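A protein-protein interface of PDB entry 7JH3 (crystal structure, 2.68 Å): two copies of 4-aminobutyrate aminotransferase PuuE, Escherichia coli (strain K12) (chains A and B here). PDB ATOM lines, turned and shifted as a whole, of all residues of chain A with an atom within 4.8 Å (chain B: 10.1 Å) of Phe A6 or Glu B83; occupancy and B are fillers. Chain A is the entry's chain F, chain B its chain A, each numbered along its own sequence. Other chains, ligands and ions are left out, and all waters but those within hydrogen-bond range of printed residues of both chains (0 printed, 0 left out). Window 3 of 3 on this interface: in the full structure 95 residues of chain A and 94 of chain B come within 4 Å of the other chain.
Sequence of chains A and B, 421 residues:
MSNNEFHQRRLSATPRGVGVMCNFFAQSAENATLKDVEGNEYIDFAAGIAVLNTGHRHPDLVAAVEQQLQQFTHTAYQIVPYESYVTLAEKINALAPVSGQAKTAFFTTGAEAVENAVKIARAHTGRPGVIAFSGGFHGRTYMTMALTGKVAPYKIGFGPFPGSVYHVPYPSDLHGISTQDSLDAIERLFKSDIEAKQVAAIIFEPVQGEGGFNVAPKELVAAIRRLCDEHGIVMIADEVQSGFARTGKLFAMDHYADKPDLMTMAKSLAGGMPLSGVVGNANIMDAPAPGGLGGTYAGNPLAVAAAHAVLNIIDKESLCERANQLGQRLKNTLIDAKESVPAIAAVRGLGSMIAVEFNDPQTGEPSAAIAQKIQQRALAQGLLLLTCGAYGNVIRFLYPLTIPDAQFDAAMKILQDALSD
Phe A6 touches just one residue of chain B: Glu B83.
Of the printed residues of chain A, Pro B81 touches Phe A25.
Printed residues of chain B within 4 Å of Phe A25: Pro B81 (3.4 Å), Tyr B82 (3.7 Å) and Glu B83 (3.97 Å).
Printed residues of chain A within 4 Å of Val B86: Arg A9 (3.9 Å) and Arg A10 (3.7 Å).
Of the printed residues of chain A, Tyr B77 touches Arg A10.
Asn A3 touches none of the printed residues of chain B.
The nearest printed residue of chain A that does not touch Glu B83 is Ser A2 (4.8 Å).
The nearest printed residue of chain A that does not touch Glu B90 is Arg A10 (5.7 Å).
Hydrophobic or aromatic side chains of chain B that line the printed part of chain A: Tyr B77, Pro B81 and Val B86.
Hydrophobic or aromatic side chains of chain A that line the printed part of chain B: Phe A6, Phe A25 and Val A37.
Along chain A the printed residues that touch a printed residue of chain B span positions 6 to 37.
Among the printed residues, Asp or Glu carboxylates within 4 Å of a Lys or Arg side-chain nitrogen of the other chain: Arg A9 with Glu B90 (2.8 Å).
The guanidinium group of Arg A9 lies within salt-bridge range of the side-chain carboxylate of Glu B90 (2.8 Å).
Among the printed residues, pairs that only touch across the chains: Phe A6 with Glu B83 (3.2 Å), Arg A10 with Tyr B77 (3.3 Å), Phe A25 with Pro B81 (3.4 Å), Val A37 with Glu B83 (3.5 Å), Phe A25 with Tyr B82 (3.7 Å), Arg A10 with Val B86 (3.7 Å), Arg A9 with Val B86 (3.9 Å) and Phe A25 with Glu B83 (3.97 Å).
The backbone carbonyl oxygen (O) of Phe A25 lies within hydrogen-bond range of the backbone NH (N) of Val A37 (3.0 Å).
The side-chain hydroxyl (OH) of Tyr B82 lies within hydrogen-bond range of the backbone carbonyl oxygen (O) of Gly B299 (2.6 Å).
The side-chain amide oxygen (OD1) of Asn A3 lies within hydrogen-bond range of the backbone NH (N) of Phe A25 (3.3 Å).
The backbone carbonyl oxygen (O) of Glu B83 lies within hydrogen-bond range of the side-chain hydroxyl (OG1) of Thr B87 (3.1 Å).
No position is printed for both chains.
Of the 9 pairs that touch across the chains among the printed residues, none has its exchanged pair printed and touching as well.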
ATOM      1  N   SER A   2     -27.918  18.468  23.198  1.00  0.00           N
ATOM      2  CA  SER A   2     -29.009  19.341  23.619  1.00  0.00           C
ATOM      3  C   SER A   2     -29.396  20.329  22.520  1.00  0.00           C
ATOM      4  O   SER A   2     -28.556  21.092  22.039  1.00  0.00           O
ATOM      5  CB  SER A   2     -28.623  20.103  24.888  1.00  0.00           C
ATOM      6  OG  SER A   2     -29.636  21.022  25.258  1.00  0.00           O
ATOM      7  N   ASN A   3     -30.677  20.328  22.138  1.00  0.00           N
ATOM      8  CA  ASN A   3     -31.129  21.222  21.074  1.00  0.00           C
ATOM      9  C   ASN A   3     -31.248  22.671  21.540  1.00  0.00           C
ATOM     10  O   ASN A   3     -31.099  23.587  20.728  1.00  0.00           O
ATOM     11  CB  ASN A   3     -32.469  20.741  20.510  1.00  0.00           C
ATOM     12  CG  ASN A   3     -32.328  19.512  19.622  1.00  0.00           C
ATOM     13  OD1 ASN A   3     -31.329  19.343  18.919  1.00  0.00           O
ATOM     14  ND2 ASN A   3     -33.335  18.650  19.648  1.00  0.00           N
ATOM     15  N   ASN A   4     -31.517  22.900  22.829  1.00  0.00           N
ATOM     16  CA  ASN A   4     -31.654  24.266  23.333  1.00  0.00           C
ATOM     17  C   ASN A   4     -30.296  24.954  23.476  1.00  0.00           C
ATOM     18  O   ASN A   4     -30.124  26.105  23.047  1.00  0.00           O
ATOM     19  CB  ASN A   4     -32.398  24.251  24.670  1.00  0.00           C
ATOM     20  CG  ASN A   4     -32.957  25.612  25.045  1.00  0.00           C
ATOM     21  OD1 ASN A   4     -32.244  26.615  25.022  1.00  0.00           O
ATOM     22  ND2 ASN A   4     -34.241  25.652  25.383  1.00  0.00           N
ATOM     23  N   GLU A   5     -29.322  24.234  24.019  1.00  0.00           N
ATOM     24  CA  GLU A   5     -27.965  24.799  24.198  1.00  0.00           C
ATOM     25  C   GLU A   5     -27.374  25.117  22.829  1.00  0.00           C
ATOM     26  O   GLU A   5     -26.797  26.168  22.683  1.00  0.00           O
ATOM     27  CB  GLU A   5     -27.107  23.904  25.091  1.00  0.00           C
ATOM     28  CG  GLU A   5     -27.616  23.868  26.522  1.00  0.00           C
ATOM     29  CD  GLU A   5     -26.893  22.957  27.505  1.00  0.00           C
ATOM     30  OE1 GLU A   5     -26.037  22.132  27.059  1.00  0.00           O
ATOM     31  OE2 GLU A   5     -27.171  23.073  28.722  1.00  0.00           O
ATOM     32  N   PHE A   6     -27.558  24.241  21.855  1.00  0.00           N
ATOM     33  CA  PHE A   6     -27.060  24.535  20.520  1.00  0.00           C
ATOM     34  C   PHE A   6     -27.934  25.540  19.779  1.00  0.00           C
ATOM     35  O   PHE A   6     -27.424  26.255  18.917  1.00  0.00           O
ATOM     36  CB  PHE A   6     -26.898  23.245  19.714  1.00  0.00           C
ATOM     37  CG  PHE A   6     -25.514  22.660  19.793  1.00  0.00           C
ATOM     38  CD1 PHE A   6     -24.492  23.160  18.999  1.00  0.00           C
ATOM     39  CD2 PHE A   6     -25.229  21.625  20.672  1.00  0.00           C
ATOM     40  CE1 PHE A   6     -23.212  22.633  19.073  1.00  0.00           C
ATOM     41  CE2 PHE A   6     -23.949  21.091  20.749  1.00  0.00           C
ATOM     42  CZ  PHE A   6     -22.940  21.598  19.949  1.00  0.00           C
ATOM     43  N   HIS A   7     -29.225  25.638  20.102  1.00  0.00           N
ATOM     44  CA  HIS A   7     -30.028  26.734  19.564  1.00  0.00           C
ATOM     45  C   HIS A   7     -29.433  28.085  19.962  1.00  0.00           C
ATOM     46  O   HIS A   7     -29.225  28.968  19.115  1.00  0.00           O
ATOM     47  CB  HIS A   7     -31.475  26.605  20.051  1.00  0.00           C
ATOM     48  CG  HIS A   7     -32.437  27.539  19.381  1.00  0.00           C
ATOM     49  ND1 HIS A   7     -33.084  28.551  20.060  1.00  0.00           N
ATOM     50  CD2 HIS A   7     -32.881  27.602  18.103  1.00  0.00           C
ATOM     51  CE1 HIS A   7     -33.876  29.203  19.228  1.00  0.00           C
ATOM     52  NE2 HIS A   7     -33.773  28.648  18.033  1.00  0.00           N
ATOM     53  N   GLN A   8     -29.121  28.248  21.253  1.00  0.00           N
ATOM     54  CA  GLN A   8     -28.513  29.499  21.704  1.00  0.00           C
ATOM     55  C   GLN A   8     -27.122  29.695  21.105  1.00  0.00           C
ATOM     56  O   GLN A   8     -26.767  30.811  20.708  1.00  0.00           O
ATOM     57  CB  GLN A   8     -28.451  29.543  23.231  1.00  0.00           C
ATOM     58  CG  GLN A   8     -27.721  30.760  23.781  1.00  0.00           C
ATOM     59  CD  GLN A   8     -28.385  32.074  23.392  1.00  0.00           C
ATOM     60  OE1 GLN A   8     -29.592  32.125  23.138  1.00  0.00           O
ATOM     61  NE2 GLN A   8     -27.595  33.144  23.342  1.00  0.00           N
ATOM     62  N   ARG A   9     -26.318  28.631  21.029  1.00  0.00           N
ATOM     63  CA  ARG A   9     -24.991  28.759  20.426  1.00  0.00           C
ATOM     64  C   ARG A   9     -25.083  29.177  18.963  1.00  0.00           C
ATOM     65  O   ARG A   9     -24.267  29.975  18.483  1.00  0.00           O
ATOM     66  CB  ARG A   9     -24.218  27.446  20.557  1.00  0.00           C
ATOM     67  CG  ARG A   9     -23.863  27.079  21.983  1.00  0.00           C
ATOM     68  CD  ARG A   9     -23.199  25.719  22.073  1.00  0.00           C
ATOM     69  NE  ARG A   9     -21.893  25.694  21.422  1.00  0.00           N
ATOM     70  CZ  ARG A   9     -21.006  24.716  21.574  1.00  0.00           C
ATOM     71  NH1 ARG A   9     -21.278  23.686  22.362  1.00  0.00           N
ATOM     72  NH2 ARG A   9     -19.840  24.772  20.943  1.00  0.00           N
ATOM     73  N   ARG A  10     -26.070  28.642  18.238  1.00  0.00           N
ATOM     74  CA  ARG A  10     -26.261  29.002  16.840  1.00  0.00           C
ATOM     75  C   ARG A  10     -26.629  30.470  16.712  1.00  0.00           C
ATOM     76  O   ARG A  10     -26.076  31.194  15.874  1.00  0.00           O
ATOM     77  CB  ARG A  10     -27.345  28.119  16.216  1.00  0.00           C
ATOM     78  CG  ARG A  10     -27.548  28.342  14.726  1.00  0.00           C
ATOM     79  CD  ARG A  10     -28.797  27.639  14.217  1.00  0.00           C
ATOM     80  NE  ARG A  10     -30.027  28.250  14.716  1.00  0.00           N
ATOM     81  CZ  ARG A  10     -30.569  29.356  14.212  1.00  0.00           C
ATOM     82  NH1 ARG A  10     -29.987  29.982  13.195  1.00  0.00           N
ATOM     83  NH2 ARG A  10     -31.693  29.842  14.725  1.00  0.00           N
ATOM     84  N   PHE A  25     -31.270  19.832  15.697  1.00  0.00           N
ATOM     85  CA  PHE A  25     -30.047  19.734  14.913  1.00  0.00           C
ATOM     86  C   PHE A  25     -29.895  18.324  14.365  1.00  0.00           C
ATOM     87  O   PHE A  25     -30.065  17.347  15.101  1.00  0.00           O
ATOM     88  CB  PHE A  25     -28.834  20.121  15.758  1.00  0.00           C
ATOM     89  CG  PHE A  25     -28.768  21.587  16.073  1.00  0.00           C
ATOM     90  CD1 PHE A  25     -29.573  22.135  17.060  1.00  0.00           C
ATOM     91  CD2 PHE A  25     -27.915  22.419  15.370  1.00  0.00           C
ATOM     92  CE1 PHE A  25     -29.523  23.480  17.340  1.00  0.00           C
ATOM     93  CE2 PHE A  25     -27.858  23.768  15.645  1.00  0.00           C
ATOM     94  CZ  PHE A  25     -28.665  24.300  16.634  1.00  0.00           C
ATOM     95  N   VAL A  37     -29.969  15.043  16.984  1.00  0.00           N
ATOM     96  CA  VAL A  37     -28.963  14.694  17.981  1.00  0.00           C
ATOM     97  C   VAL A  37     -29.558  14.107  19.249  1.00  0.00           C
ATOM     98  O   VAL A  37     -28.810  13.611  20.097  1.00  0.00           O
ATOM     99  CB  VAL A  37     -28.102  15.922  18.346  1.00  0.00           C
ATOM    100  CG1 VAL A  37     -27.359  16.427  17.127  1.00  0.00           C
ATOM    101  CG2 VAL A  37     -28.965  17.026  18.941  1.00  0.00           C
ATOM    102  N   GLN B  68     -18.282  12.191   7.825  1.00  0.00           N
ATOM    103  CA  GLN B  68     -19.551  12.948   7.695  1.00  0.00           C
ATOM    104  C   GLN B  68     -20.434  12.245   6.674  1.00  0.00           C
ATOM    105  O   GLN B  68     -21.624  12.125   6.883  1.00  0.00           O
ATOM    106  CB  GLN B  68     -19.274  14.407   7.330  1.00  0.00           C
ATOM    107  CG  GLN B  68     -20.509  15.274   7.143  1.00  0.00           C
ATOM    108  CD  GLN B  68     -21.494  15.291   8.279  1.00  0.00           C
ATOM    109  OE1 GLN B  68     -21.143  15.370   9.435  1.00  0.00           O
ATOM    110  NE2 GLN B  68     -22.758  15.222   7.951  1.00  0.00           N
ATOM    111  N   GLN B  71     -22.921  10.229   7.792  1.00  0.00           N
ATOM    112  CA  GLN B  71     -24.013  10.860   8.529  1.00  0.00           C
ATOM    113  C   GLN B  71     -25.043  11.495   7.602  1.00  0.00           C
ATOM    114  O   GLN B  71     -26.199  11.059   7.576  1.00  0.00           O
ATOM    115  CB  GLN B  71     -23.467  11.909   9.512  1.00  0.00           C
ATOM    116  CG  GLN B  71     -22.370  11.405  10.443  1.00  0.00           C
ATOM    117  CD  GLN B  71     -22.749  10.126  11.168  1.00  0.00           C
ATOM    118  OE1 GLN B  71     -23.905   9.929  11.549  1.00  0.00           O
ATOM    119  NE2 GLN B  71     -21.774   9.244  11.355  1.00  0.00           N
ATOM    120  N   PHE B  72     -24.659  12.529   6.854  1.00  0.00           N
ATOM    121  CA  PHE B  72     -25.528  13.193   5.889  1.00  0.00           C
ATOM    122  C   PHE B  72     -24.687  14.159   5.068  1.00  0.00           C
ATOM    123  O   PHE B  72     -23.694  14.707   5.559  1.00  0.00           O
ATOM    124  CB  PHE B  72     -26.688  13.940   6.570  1.00  0.00           C
ATOM    125  CG  PHE B  72     -26.249  14.942   7.599  1.00  0.00           C
ATOM    126  CD1 PHE B  72     -26.031  14.554   8.910  1.00  0.00           C
ATOM    127  CD2 PHE B  72     -26.063  16.274   7.258  1.00  0.00           C
ATOM    128  CE1 PHE B  72     -25.628  15.472   9.860  1.00  0.00           C
ATOM    129  CE2 PHE B  72     -25.659  17.198   8.207  1.00  0.00           C
ATOM    130  CZ  PHE B  72     -25.442  16.797   9.508  1.00  0.00           C
ATOM    131  N   THR B  75     -28.764  18.842   4.295  1.00  0.00           N
ATOM    132  CA  THR B  75     -30.094  18.967   4.863  1.00  0.00           C
ATOM    133  C   THR B  75     -30.756  20.288   4.516  1.00  0.00           C
ATOM    134  O   THR B  75     -31.919  20.489   4.884  1.00  0.00           O
ATOM    135  CB  THR B  75     -30.042  18.823   6.388  1.00  0.00           C
ATOM    136  OG1 THR B  75     -29.241  19.880   6.931  1.00  0.00           O
ATOM    137  CG2 THR B  75     -29.451  17.481   6.784  1.00  0.00           C
ATOM    138  N   TYR B  77     -29.237  23.960   5.330  1.00  0.00           N
ATOM    139  CA  TYR B  77     -29.003  24.504   6.663  1.00  0.00           C
ATOM    140  C   TYR B  77     -30.145  25.404   7.109  1.00  0.00           C
ATOM    141  O   TYR B  77     -30.566  25.353   8.271  1.00  0.00           O
ATOM    142  CB  TYR B  77     -27.681  25.265   6.687  1.00  0.00           C
ATOM    143  CG  TYR B  77     -27.399  25.937   8.005  1.00  0.00           C
ATOM    144  CD1 TYR B  77     -26.876  25.222   9.073  1.00  0.00           C
ATOM    145  CD2 TYR B  77     -27.651  27.289   8.181  1.00  0.00           C
ATOM    146  CE1 TYR B  77     -26.615  25.836  10.277  1.00  0.00           C
ATOM    147  CE2 TYR B  77     -27.394  27.911   9.381  1.00  0.00           C
ATOM    148  CZ  TYR B  77     -26.876  27.181  10.426  1.00  0.00           C
ATOM    149  OH  TYR B  77     -26.618  27.805  11.625  1.00  0.00           O
ATOM    150  N   VAL B  80     -32.856  22.602   8.309  1.00  0.00           N
ATOM    151  CA  VAL B  80     -32.405  21.852   9.474  1.00  0.00           C
ATOM    152  C   VAL B  80     -30.920  22.129   9.683  1.00  0.00           C
ATOM    153  O   VAL B  80     -30.094  21.757   8.842  1.00  0.00           O
ATOM    154  CB  VAL B  80     -32.660  20.341   9.330  1.00  0.00           C
ATOM    155  CG1 VAL B  80     -32.150  19.600  10.559  1.00  0.00           C
ATOM    156  CG2 VAL B  80     -34.141  20.073   9.117  1.00  0.00           C
ATOM    157  N   PRO B  81     -30.535  22.761  10.785  1.00  0.00           N
ATOM    158  CA  PRO B  81     -29.127  23.080  11.027  1.00  0.00           C
ATOM    159  C   PRO B  81     -28.399  21.882  11.629  1.00  0.00           C
ATOM    160  O   PRO B  81     -28.984  20.839  11.913  1.00  0.00           O
ATOM    161  CB  PRO B  81     -29.211  24.242  12.014  1.00  0.00           C
ATOM    162  CG  PRO B  81     -30.435  23.932  12.812  1.00  0.00           C
ATOM    163  CD  PRO B  81     -31.405  23.265  11.862  1.00  0.00           C
ATOM    164  N   TYR B  82     -27.095  22.051  11.826  1.00  0.00           N
ATOM    165  CA  TYR B  82     -26.257  20.980  12.338  1.00  0.00           C
ATOM    166  C   TYR B  82     -25.112  21.600  13.121  1.00  0.00           C
ATOM    167  O   TYR B  82     -24.747  22.758  12.910  1.00  0.00           O
ATOM    168  CB  TYR B  82     -25.739  20.073  11.208  1.00  0.00           C
ATOM    169  CG  TYR B  82     -25.647  20.734   9.844  1.00  0.00           C
ATOM    170  CD1 TYR B  82     -26.764  20.836   9.021  1.00  0.00           C
ATOM    171  CD2 TYR B  82     -24.437  21.228   9.369  1.00  0.00           C
ATOM    172  CE1 TYR B  82     -26.683  21.431   7.776  1.00  0.00           C
ATOM    173  CE2 TYR B  82     -24.346  21.821   8.118  1.00  0.00           C
ATOM    174  CZ  TYR B  82     -25.474  21.920   7.328  1.00  0.00           C
ATOM    175  OH  TYR B  82     -25.396  22.509   6.084  1.00  0.00           O
ATOM    176  N   GLU B  83     -24.542  20.808  14.034  1.00  0.00           N
ATOM    177  CA  GLU B  83     -23.616  21.363  15.015  1.00  0.00           C
ATOM    178  C   GLU B  83     -22.240  21.664  14.432  1.00  0.00           C
ATOM    179  O   GLU B  83     -21.523  22.510  14.981  1.00  0.00           O
ATOM    180  CB  GLU B  83     -23.499  20.412  16.204  1.00  0.00           C
ATOM    181  CG  GLU B  83     -24.833  20.149  16.902  1.00  0.00           C
ATOM    182  CD  GLU B  83     -24.699  19.217  18.092  1.00  0.00           C
ATOM    183  OE1 GLU B  83     -23.599  18.654  18.286  1.00  0.00           O
ATOM    184  OE2 GLU B  83     -25.692  19.050  18.835  1.00  0.00           O
ATOM    185  N   SER B  84     -21.856  21.004  13.337  1.00  0.00           N
ATOM    186  CA  SER B  84     -20.556  21.278  12.728  1.00  0.00           C
ATOM    187  C   SER B  84     -20.496  22.696  12.173  1.00  0.00           C
ATOM    188  O   SER B  84     -19.470  23.375  12.298  1.00  0.00           O
ATOM    189  CB  SER B  84     -20.269  20.255  11.631  1.00  0.00           C
ATOM    190  OG  SER B  84     -21.246  20.333  10.608  1.00  0.00           O
ATOM    191  N   TYR B  85     -21.586  23.151  11.550  1.00  0.00           N
ATOM    192  CA  TYR B  85     -21.699  24.541  11.117  1.00  0.00           C
ATOM    193  C   TYR B  85     -21.441  25.496  12.279  1.00  0.00           C
ATOM    194  O   TYR B  85     -20.633  26.427  12.168  1.00  0.00           O
ATOM    195  CB  TYR B  85     -23.092  24.766  10.517  1.00  0.00           C
ATOM    196  CG  TYR B  85     -23.347  26.097   9.831  1.00  0.00           C
ATOM    197  CD1 TYR B  85     -23.502  27.269  10.564  1.00  0.00           C
ATOM    198  CD2 TYR B  85     -23.493  26.168   8.450  1.00  0.00           C
ATOM    199  CE1 TYR B  85     -23.755  28.478   9.938  1.00  0.00           C
ATOM    200  CE2 TYR B  85     -23.751  27.374   7.814  1.00  0.00           C
ATOM    201  CZ  TYR B  85     -23.880  28.526   8.563  1.00  0.00           C
ATOM    202  OH  TYR B  85     -24.136  29.727   7.937  1.00  0.00           O
ATOM    203  N   VAL B  86     -22.109  25.266  13.412  1.00  0.00           N
ATOM    204  CA  VAL B  86     -22.000  26.188  14.539  1.00  0.00           C
ATOM    205  C   VAL B  86     -20.594  26.163  15.127  1.00  0.00           C
ATOM    206  O   VAL B  86     -20.033  27.213  15.461  1.00  0.00           O
ATOM    207  CB  VAL B  86     -23.063  25.865  15.603  1.00  0.00           C
ATOM    208  CG1 VAL B  86     -22.867  26.745  16.825  1.00  0.00           C
ATOM    209  CG2 VAL B  86     -24.456  26.049  15.033  1.00  0.00           C
ATOM    210  N   THR B  87     -19.997  24.976  15.265  1.00  0.00           N
ATOM    211  CA  THR B  87     -18.663  24.913  15.855  1.00  0.00           C
ATOM    212  C   THR B  87     -17.616  25.521  14.926  1.00  0.00           C
ATOM    213  O   THR B  87     -16.662  26.166  15.389  1.00  0.00           O
ATOM    214  CB  THR B  87     -18.301  23.472  16.214  1.00  0.00           C
ATOM    215  OG1 THR B  87     -18.463  22.627  15.068  1.00  0.00           O
ATOM    216  CG2 THR B  87     -19.190  22.968  17.331  1.00  0.00           C
ATOM    217  N   LEU B  88     -17.780  25.349  13.613  1.00  0.00           N
ATOM    218  CA  LEU B  88     -16.864  25.999  12.683  1.00  0.00           C
ATOM    219  C   LEU B  88     -17.028  27.511  12.736  1.00  0.00           C
ATOM    220  O   LEU B  88     -16.039  28.253  12.693  1.00  0.00           O
ATOM    221  CB  LEU B  88     -17.089  25.471  11.265  1.00  0.00           C
ATOM    222  CG  LEU B  88     -16.058  25.909  10.225  1.00  0.00           C
ATOM    223  CD1 LEU B  88     -14.665  25.430  10.601  1.00  0.00           C
ATOM    224  CD2 LEU B  88     -16.450  25.408   8.848  1.00  0.00           C
ATOM    225  N   ALA B  89     -18.272  27.986  12.841  1.00  0.00           N
ATOM    226  CA  ALA B  89     -18.501  29.416  13.005  1.00  0.00           C
ATOM    227  C   ALA B  89     -17.826  29.937  14.267  1.00  0.00           C
ATOM    228  O   ALA B  89     -17.226  31.016  14.256  1.00  0.00           O
ATOM    229  CB  ALA B  89     -19.998  29.712  13.041  1.00  0.00           C
ATOM    230  N   GLU B  90     -17.912  29.182  15.362  1.00  0.00           N
ATOM    231  CA  GLU B  90     -17.305  29.618  16.616  1.00  0.00           C
ATOM    232  C   GLU B  90     -15.788  29.696  16.499  1.00  0.00           C
ATOM    233  O   GLU B  90     -15.167  30.663  16.963  1.00  0.00           O
ATOM    234  CB  GLU B  90     -17.712  28.674  17.747  1.00  0.00           C
ATOM    235  CG  GLU B  90     -19.180  28.766  18.131  1.00  0.00           C
ATOM    236  CD  GLU B  90     -19.608  27.657  19.070  1.00  0.00           C
ATOM    237  OE1 GLU B  90     -18.882  26.645  19.159  1.00  0.00           O
ATOM    238  OE2 GLU B  90     -20.668  27.795  19.718  1.00  0.00           O
ATOM    239  N   LYS B  91     -15.173  28.690  15.868  1.00  0.00           N
ATOM    240  CA  LYS B  91     -13.727  28.728  15.671  1.00  0.00           C
ATOM    241  C   LYS B  91     -13.318  29.911  14.797  1.00  0.00           C
ATOM    242  O   LYS B  91     -12.346  30.617  15.106  1.00  0.00           O
ATOM    243  CB  LYS B  91     -13.240  27.412  15.063  1.00  0.00           C
ATOM    244  CG  LYS B  91     -13.509  26.191  15.933  1.00  0.00           C
ATOM    245  CD  LYS B  91     -12.899  24.926  15.333  1.00  0.00           C
ATOM    246  CE  LYS B  91     -13.227  23.691  16.163  1.00  0.00           C
ATOM    247  NZ  LYS B  91     -12.640  22.449  15.585  1.00  0.00           N
ATOM    248  N   PHE B 106     -21.842  30.918   6.583  1.00  0.00           N
ATOM    249  CA  PHE B 106     -21.220  30.091   5.561  1.00  0.00           C
ATOM    250  C   PHE B 106     -22.071  30.068   4.302  1.00  0.00           C
ATOM    251  O   PHE B 106     -23.305  30.095   4.366  1.00  0.00           O
ATOM    252  CB  PHE B 106     -20.992  28.666   6.068  1.00  0.00           C
ATOM    253  CG  PHE B 106     -19.966  28.579   7.153  1.00  0.00           C
ATOM    254  CD1 PHE B 106     -18.646  28.910   6.898  1.00  0.00           C
ATOM    255  CD2 PHE B 106     -20.315  28.177   8.428  1.00  0.00           C
ATOM    256  CE1 PHE B 106     -17.698  28.841   7.891  1.00  0.00           C
ATOM    257  CE2 PHE B 106     -19.369  28.106   9.422  1.00  0.00           C
ATOM    258  CZ  PHE B 106     -18.061  28.443   9.152  1.00  0.00           C
ATOM    259  N   GLY B 299     -22.875  26.160   3.451  1.00  0.00           N
ATOM    260  CA  GLY B 299     -22.365  25.431   4.596  1.00  0.00           C
ATOM    261  C   GLY B 299     -22.559  23.937   4.458  1.00  0.00           C
ATOM    262  O   GLY B 299     -23.024  23.276   5.393  1.00  0.00           O
ATOM    263  N   PRO B 301     -22.422  20.148   4.658  1.00  0.00           N
ATOM    264  CA  PRO B 301     -21.833  19.374   5.770  1.00  0.00           C
ATOM    265  C   PRO B 301     -20.463  18.772   5.487  1.00  0.00           C
ATOM    266  O   PRO B 301     -19.574  18.847   6.347  1.00  0.00           O
ATOM    267  CB  PRO B 301     -22.886  18.284   6.008  1.00  0.00           C
ATOM    268  CG  PRO B 301     -24.174  18.933   5.604  1.00  0.00           C
ATOM    269  CD  PRO B 301     -23.850  19.848   4.456  1.00  0.00           C
ATOM    270  N   VAL B 304     -17.931  21.457   5.523  1.00  0.00           N
ATOM    271  CA  VAL B 304     -17.724  21.957   6.879  1.00  0.00           C
ATOM    272  C   VAL B 304     -16.816  21.016   7.665  1.00  0.00           C
ATOM    273  O   VAL B 304     -15.909  21.459   8.389  1.00  0.00           O
ATOM    274  CB  VAL B 304     -19.082  22.163   7.573  1.00  0.00           C
ATOM    275  CG1 VAL B 304     -18.892  22.437   9.053  1.00  0.00           C
ATOM    276  CG2 VAL B 304     -19.841  23.306   6.910  1.00  0.00           C
ATOM    277  N   ALA B 305     -17.042  19.706   7.540  1.00  0.00           N
ATOM    278  CA  ALA B 305     -16.136  18.744   8.159  1.00  0.00           C
ATOM    279  C   ALA B 305     -14.721  18.910   7.622  1.00  0.00           C
ATOM    280  O   ALA B 305     -13.743  18.891   8.386  1.00  0.00           O
ATOM    281  CB  ALA B 305     -16.641  17.320   7.922  1.00  0.00           C
ATOM    282  N   HIS B 308     -13.113  21.957   9.282  1.00  0.00           N
ATOM    283  CA  HIS B 308     -12.632  21.565  10.606  1.00  0.00           C
ATOM    284  C   HIS B 308     -11.275  20.887  10.496  1.00  0.00           C
ATOM    285  O   HIS B 308     -10.304  21.263  11.176  1.00  0.00           O
ATOM    286  CB  HIS B 308     -13.631  20.622  11.282  1.00  0.00           C
ATOM    287  CG  HIS B 308     -14.736  21.322  12.009  1.00  0.00           C
ATOM    288  ND1 HIS B 308     -14.533  22.012  13.186  1.00  0.00           N
ATOM    289  CD2 HIS B 308     -16.058  21.431  11.734  1.00  0.00           C
ATOM    290  CE1 HIS B 308     -15.679  22.523  13.597  1.00  0.00           C
ATOM    291  NE2 HIS B 308     -16.621  22.185  12.734  1.00  0.00           N
